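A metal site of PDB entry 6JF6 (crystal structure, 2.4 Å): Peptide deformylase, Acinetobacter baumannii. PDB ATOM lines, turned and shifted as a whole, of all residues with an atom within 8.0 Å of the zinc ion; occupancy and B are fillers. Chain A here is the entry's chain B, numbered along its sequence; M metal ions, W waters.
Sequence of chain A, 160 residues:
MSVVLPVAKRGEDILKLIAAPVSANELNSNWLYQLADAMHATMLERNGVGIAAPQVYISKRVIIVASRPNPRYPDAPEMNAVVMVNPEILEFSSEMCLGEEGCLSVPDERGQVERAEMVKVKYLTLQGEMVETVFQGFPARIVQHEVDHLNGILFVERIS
The side-chain carboxylate (OE1) of Glu 101 is in hydrogen-bond range of a ring nitrogen (ND1) of His 145. OE1 of Gln 55 sits close to NE2 of His 149 (3.5 Å). The side-chain sulfur (SG) of Cys 103 sits close to the side-chain amide nitrogen (NE2) of Gln 55 (3.5 Å). The backbone NH (N) of Ser 105 sits close to the side-chain sulfur (SG) of Cys 103, at 3.5 Å. The side-chain carboxylate (OE1) of Glu 146 sits close to the side-chain amide oxygen (OE1) of Gln 55 (3.4 Å). The side-chain amide nitrogen (NE2) of Gln 55 is in hydrogen-bond range of the side-chain hydroxyl (OG) of Ser 105. N of Ala 52 sits at hydrogen-bond distance from OE1 of Gln 55, at 3.1 Å.
Gln 55 touches the zinc ion. Of the 21 residues printed, 4 come within 4 Å of the zinc ion.
The zinc ion is bound by NE2 of His 145, NE2 of His 149, SG of Cys 103 and water W1.
Water W1 bridges the side-chain amide oxygen of Gln 55 and the side-chain carboxylate of Glu 146. Water W3 lies within hydrogen-bond range of the backbone NH (N) of Leu 104 and the side-chain amide nitrogen (NE2) of Gln 55.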
ATOM      1  N   LEU A  15       0.307 -16.419 -27.082  1.00  0.00           N
ATOM      2  CA  LEU A  15       1.133 -16.686 -25.893  1.00  0.00           C
ATOM      3  C   LEU A  15       2.607 -16.313 -26.078  1.00  0.00           C
ATOM      4  O   LEU A  15       3.372 -16.426 -25.090  1.00  0.00           O
ATOM      5  CB  LEU A  15       1.056 -18.195 -25.517  1.00  0.00           C
ATOM      6  CG  LEU A  15      -0.053 -18.921 -24.731  1.00  0.00           C
ATOM      7  CD1 LEU A  15      -1.215 -18.060 -24.297  1.00  0.00           C
ATOM      8  CD2 LEU A  15      -0.504 -20.187 -25.493  1.00  0.00           C
ATOM      9  N   GLY A  50      -3.683 -18.752 -10.311  1.00  0.00           N
ATOM     10  CA  GLY A  50      -3.480 -17.469 -10.947  1.00  0.00           C
ATOM     11  C   GLY A  50      -3.874 -17.564 -12.399  1.00  0.00           C
ATOM     12  O   GLY A  50      -4.072 -18.644 -12.925  1.00  0.00           O
ATOM     13  N   ILE A  51      -3.925 -16.428 -13.057  1.00  0.00           N
ATOM     14  CA  ILE A  51      -4.216 -16.439 -14.491  1.00  0.00           C
ATOM     15  C   ILE A  51      -3.714 -15.172 -15.111  1.00  0.00           C
ATOM     16  O   ILE A  51      -3.563 -14.160 -14.429  1.00  0.00           O
ATOM     17  CB  ILE A  51      -5.728 -16.639 -14.752  1.00  0.00           C
ATOM     18  CG1 ILE A  51      -5.967 -17.113 -16.192  1.00  0.00           C
ATOM     19  CG2 ILE A  51      -6.506 -15.368 -14.377  1.00  0.00           C
ATOM     20  CD1 ILE A  51      -7.381 -17.579 -16.455  1.00  0.00           C
ATOM     21  N   ALA A  52      -3.442 -15.232 -16.405  1.00  0.00           N
ATOM     22  CA  ALA A  52      -2.928 -14.075 -17.147  1.00  0.00           C
ATOM     23  C   ALA A  52      -3.764 -13.827 -18.421  1.00  0.00           C
ATOM     24  O   ALA A  52      -4.103 -14.749 -19.173  1.00  0.00           O
ATOM     25  CB  ALA A  52      -1.456 -14.322 -17.473  1.00  0.00           C
ATOM     26  N   GLN A  55      -3.690 -15.734 -21.844  1.00  0.00           N
ATOM     27  CA  GLN A  55      -4.210 -17.099 -21.890  1.00  0.00           C
ATOM     28  C   GLN A  55      -5.669 -17.111 -22.397  1.00  0.00           C
ATOM     29  O   GLN A  55      -6.124 -18.137 -22.925  1.00  0.00           O
ATOM     30  CB  GLN A  55      -4.100 -17.789 -20.498  1.00  0.00           C
ATOM     31  CG  GLN A  55      -2.681 -18.036 -19.956  1.00  0.00           C
ATOM     32  CD  GLN A  55      -2.653 -18.672 -18.554  1.00  0.00           C
ATOM     33  OE1 GLN A  55      -2.508 -17.972 -17.541  1.00  0.00           O
ATOM     34  NE2 GLN A  55      -2.826 -20.005 -18.494  1.00  0.00           N
ATOM     35  N   GLU A 101       4.990 -26.416 -10.788  1.00  0.00           N
ATOM     36  CA  GLU A 101       4.085 -25.585 -11.549  1.00  0.00           C
ATOM     37  C   GLU A 101       3.321 -26.373 -12.644  1.00  0.00           C
ATOM     38  O   GLU A 101       3.821 -27.359 -13.195  1.00  0.00           O
ATOM     39  CB  GLU A 101       4.854 -24.432 -12.163  1.00  0.00           C
ATOM     40  CG  GLU A 101       5.052 -23.314 -11.154  1.00  0.00           C
ATOM     41  CD  GLU A 101       5.901 -22.195 -11.696  1.00  0.00           C
ATOM     42  OE1 GLU A 101       5.532 -21.602 -12.725  1.00  0.00           O
ATOM     43  OE2 GLU A 101       6.951 -21.951 -11.110  1.00  0.00           O
ATOM     44  N   GLY A 102       2.093 -25.927 -12.895  1.00  0.00           N
ATOM     45  CA  GLY A 102       1.339 -26.265 -14.082  1.00  0.00           C
ATOM     46  C   GLY A 102       0.648 -25.035 -14.615  1.00  0.00           C
ATOM     47  O   GLY A 102       0.613 -23.984 -13.950  1.00  0.00           O
ATOM     48  N   CYS A 103       0.106 -25.173 -15.825  1.00  0.00           N
ATOM     49  CA  CYS A 103      -0.480 -24.069 -16.561  1.00  0.00           C
ATOM     50  C   CYS A 103      -1.608 -24.558 -17.429  1.00  0.00           C
ATOM     51  O   CYS A 103      -1.388 -25.489 -18.251  1.00  0.00           O
ATOM     52  CB  CYS A 103       0.574 -23.431 -17.445  1.00  0.00           C
ATOM     53  SG  CYS A 103       0.030 -21.938 -18.247  1.00  0.00           S
ATOM     54  N   LEU A 104      -2.794 -23.956 -17.282  1.00  0.00           N
ATOM     55  CA  LEU A 104      -3.911 -24.245 -18.194  1.00  0.00           C
ATOM     56  C   LEU A 104      -3.531 -24.190 -19.685  1.00  0.00           C
ATOM     57  O   LEU A 104      -4.076 -24.940 -20.507  1.00  0.00           O
ATOM     58  CB  LEU A 104      -5.083 -23.313 -17.943  1.00  0.00           C
ATOM     59  CG  LEU A 104      -5.818 -23.619 -16.639  1.00  0.00           C
ATOM     60  CD1 LEU A 104      -6.843 -22.534 -16.379  1.00  0.00           C
ATOM     61  CD2 LEU A 104      -6.464 -25.006 -16.711  1.00  0.00           C
ATOM     62  N   SER A 105      -2.579 -23.338 -20.018  1.00  0.00           N
ATOM     63  CA  SER A 105      -2.027 -23.263 -21.371  1.00  0.00           C
ATOM     64  C   SER A 105      -1.011 -24.337 -21.760  1.00  0.00           C
ATOM     65  O   SER A 105      -0.590 -24.395 -22.916  1.00  0.00           O
ATOM     66  CB  SER A 105      -1.445 -21.871 -21.580  1.00  0.00           C
ATOM     67  OG  SER A 105      -2.423 -20.930 -21.169  1.00  0.00           O
ATOM     68  N   VAL A 106      -0.620 -25.181 -20.794  1.00  0.00           N
ATOM     69  CA  VAL A 106       0.309 -26.321 -21.040  1.00  0.00           C
ATOM     70  C   VAL A 106      -0.281 -27.623 -20.477  1.00  0.00           C
ATOM     71  O   VAL A 106       0.083 -28.056 -19.385  1.00  0.00           O
ATOM     72  CB  VAL A 106       1.717 -26.086 -20.434  1.00  0.00           C
ATOM     73  CG1 VAL A 106       2.717 -27.018 -21.091  1.00  0.00           C
ATOM     74  CG2 VAL A 106       2.164 -24.637 -20.606  1.00  0.00           C
ATOM     75  N   ARG A 115      12.376 -20.419  -9.157  1.00  0.00           N
ATOM     76  CA  ARG A 115      11.902 -19.043  -9.012  1.00  0.00           C
ATOM     77  C   ARG A 115      12.624 -18.293  -7.908  1.00  0.00           C
ATOM     78  O   ARG A 115      13.028 -18.898  -6.920  1.00  0.00           O
ATOM     79  CB  ARG A 115      10.417 -19.056  -8.686  1.00  0.00           C
ATOM     80  CG  ARG A 115       9.572 -19.680  -9.802  1.00  0.00           C
ATOM     81  CD  ARG A 115       9.553 -18.884 -11.114  1.00  0.00           C
ATOM     82  NE  ARG A 115       8.525 -19.428 -12.023  1.00  0.00           N
ATOM     83  CZ  ARG A 115       8.173 -18.925 -13.209  1.00  0.00           C
ATOM     84  NH1 ARG A 115       8.735 -17.822 -13.696  1.00  0.00           N
ATOM     85  NH2 ARG A 115       7.237 -19.535 -13.930  1.00  0.00           N
ATOM     86  N   ILE A 142       3.640 -17.410  -8.180  1.00  0.00           N
ATOM     87  CA  ILE A 142       2.471 -17.156  -9.050  1.00  0.00           C
ATOM     88  C   ILE A 142       2.660 -15.862  -9.847  1.00  0.00           C
ATOM     89  O   ILE A 142       2.461 -15.858 -11.058  1.00  0.00           O
ATOM     90  CB  ILE A 142       1.135 -17.098  -8.238  1.00  0.00           C
ATOM     91  CG1 ILE A 142       0.835 -18.446  -7.565  1.00  0.00           C
ATOM     92  CG2 ILE A 142      -0.056 -16.753  -9.138  1.00  0.00           C
ATOM     93  CD1 ILE A 142      -0.243 -18.373  -6.490  1.00  0.00           C
ATOM     94  N   HIS A 145       5.099 -16.292 -12.630  1.00  0.00           N
ATOM     95  CA  HIS A 145       4.499 -17.129 -13.685  1.00  0.00           C
ATOM     96  C   HIS A 145       3.587 -16.307 -14.634  1.00  0.00           C
ATOM     97  O   HIS A 145       3.788 -16.284 -15.879  1.00  0.00           O
ATOM     98  CB  HIS A 145       3.751 -18.293 -13.027  1.00  0.00           C
ATOM     99  CG  HIS A 145       3.136 -19.259 -13.989  1.00  0.00           C
ATOM    100  ND1 HIS A 145       3.619 -20.536 -14.170  1.00  0.00           N
ATOM    101  CD2 HIS A 145       2.049 -19.150 -14.792  1.00  0.00           C
ATOM    102  CE1 HIS A 145       2.878 -21.165 -15.058  1.00  0.00           C
ATOM    103  NE2 HIS A 145       1.911 -20.353 -15.452  1.00  0.00           N
ATOM    104  N   GLU A 146       2.662 -15.569 -14.032  1.00  0.00           N
ATOM    105  CA  GLU A 146       1.696 -14.785 -14.799  1.00  0.00           C
ATOM    106  C   GLU A 146       2.337 -13.595 -15.469  1.00  0.00           C
ATOM    107  O   GLU A 146       1.866 -13.157 -16.529  1.00  0.00           O
ATOM    108  CB  GLU A 146       0.534 -14.317 -13.905  1.00  0.00           C
ATOM    109  CG  GLU A 146      -0.144 -15.385 -13.033  1.00  0.00           C
ATOM    110  CD  GLU A 146      -0.586 -16.631 -13.800  1.00  0.00           C
ATOM    111  OE1 GLU A 146      -0.768 -16.558 -15.028  1.00  0.00           O
ATOM    112  OE2 GLU A 146      -0.776 -17.685 -13.162  1.00  0.00           O
ATOM    113  N   VAL A 147       3.416 -13.053 -14.878  1.00  0.00           N
ATOM    114  CA  VAL A 147       4.143 -11.948 -15.505  1.00  0.00           C
ATOM    115  C   VAL A 147       4.892 -12.474 -16.718  1.00  0.00           C
ATOM    116  O   VAL A 147       4.749 -11.933 -17.829  1.00  0.00           O
ATOM    117  CB  VAL A 147       5.094 -11.250 -14.497  1.00  0.00           C
ATOM    118  CG1 VAL A 147       6.167 -10.433 -15.184  1.00  0.00           C
ATOM    119  CG2 VAL A 147       4.266 -10.388 -13.559  1.00  0.00           C
ATOM    120  N   ASP A 148       5.624 -13.565 -16.537  1.00  0.00           N
ATOM    121  CA  ASP A 148       6.134 -14.309 -17.714  1.00  0.00           C
ATOM    122  C   ASP A 148       5.181 -14.416 -18.917  1.00  0.00           C
ATOM    123  O   ASP A 148       5.616 -14.295 -20.041  1.00  0.00           O
ATOM    124  CB  ASP A 148       6.542 -15.713 -17.300  1.00  0.00           C
ATOM    125  CG  ASP A 148       7.874 -15.745 -16.618  1.00  0.00           C
ATOM    126  OD1 ASP A 148       8.544 -14.679 -16.534  1.00  0.00           O
ATOM    127  OD2 ASP A 148       8.235 -16.837 -16.172  1.00  0.00           O
ATOM    128  N   HIS A 149       3.890 -14.639 -18.651  1.00  0.00           N
ATOM    129  CA  HIS A 149       2.830 -14.761 -19.688  1.00  0.00           C
ATOM    130  C   HIS A 149       2.662 -13.458 -20.461  1.00  0.00           C
ATOM    131  O   HIS A 149       2.462 -13.474 -21.695  1.00  0.00           O
ATOM    132  CB  HIS A 149       1.477 -15.182 -19.038  1.00  0.00           C
ATOM    133  CG  HIS A 149       1.230 -16.661 -18.979  1.00  0.00           C
ATOM    134  ND1 HIS A 149       1.088 -17.452 -20.108  1.00  0.00           N
ATOM    135  CD2 HIS A 149       1.013 -17.484 -17.930  1.00  0.00           C
ATOM    136  CE1 HIS A 149       0.801 -18.690 -19.753  1.00  0.00           C
ATOM    137  NE2 HIS A 149       0.761 -18.741 -18.433  1.00  0.00           N
ATOM    138  N   ILE A 153       6.207 -15.761 -22.357  1.00  0.00           N
ATOM    139  CA  ILE A 153       7.068 -16.829 -21.814  1.00  0.00           C
ATOM    140  C   ILE A 153       6.196 -17.827 -21.044  1.00  0.00           C
ATOM    141  O   ILE A 153       5.446 -17.430 -20.149  1.00  0.00           O
ATOM    142  CB  ILE A 153       8.185 -16.280 -20.884  1.00  0.00           C
ATOM    143  CG1 ILE A 153       9.261 -15.583 -21.710  1.00  0.00           C
ATOM    144  CG2 ILE A 153       8.838 -17.408 -20.104  1.00  0.00           C
ATOM    145  CD1 ILE A 153      10.109 -14.608 -20.933  1.00  0.00           C
ATOM    146  N   LEU A 154       6.279 -19.092 -21.460  1.00  0.00           N
ATOM    147  CA  LEU A 154       5.659 -20.223 -20.753  1.00  0.00           C
ATOM    148  C   LEU A 154       6.650 -20.899 -19.795  1.00  0.00           C
ATOM    149  O   LEU A 154       7.844 -20.991 -20.110  1.00  0.00           O
ATOM    150  CB  LEU A 154       5.198 -21.238 -21.783  1.00  0.00           C
ATOM    151  CG  LEU A 154       4.123 -20.798 -22.751  1.00  0.00           C
ATOM    152  CD1 LEU A 154       3.761 -21.958 -23.701  1.00  0.00           C
ATOM    153  CD2 LEU A 154       2.909 -20.286 -21.987  1.00  0.00           C
ATOM    154  N   PHE A 155       6.150 -21.407 -18.671  1.00  0.00           N
ATOM    155  CA  PHE A 155       7.019 -21.956 -17.613  1.00  0.00           C
ATOM    156  C   PHE A 155       8.018 -23.009 -18.082  1.00  0.00           C
ATOM    157  O   PHE A 155       9.138 -23.039 -17.596  1.00  0.00           O
ATOM    158  CB  PHE A 155       6.214 -22.478 -16.403  1.00  0.00           C
ATOM    159  CG  PHE A 155       5.609 -23.838 -16.619  1.00  0.00           C
ATOM    160  CD1 PHE A 155       4.420 -23.984 -17.288  1.00  0.00           C
ATOM    161  CD2 PHE A 155       6.240 -24.994 -16.143  1.00  0.00           C
ATOM    162  CE1 PHE A 155       3.877 -25.246 -17.500  1.00  0.00           C
ATOM    163  CE2 PHE A 155       5.703 -26.247 -16.345  1.00  0.00           C
ATOM    164  CZ  PHE A 155       4.511 -26.373 -17.024  1.00  0.00           C
HETATM  165 ZN    ZN M   1       0.374 -20.138 -16.799  1.00  0.00          ZN
HETATM  166  O   HOH W   1      -1.455 -19.284 -15.579  1.00  0.00           O
HETATM  167  O   HOH W   2       2.969 -20.800 -18.299  1.00  0.00           O
HETATM  168  O   HOH W   3      -2.725 -21.510 -15.933  1.00  0.00           O
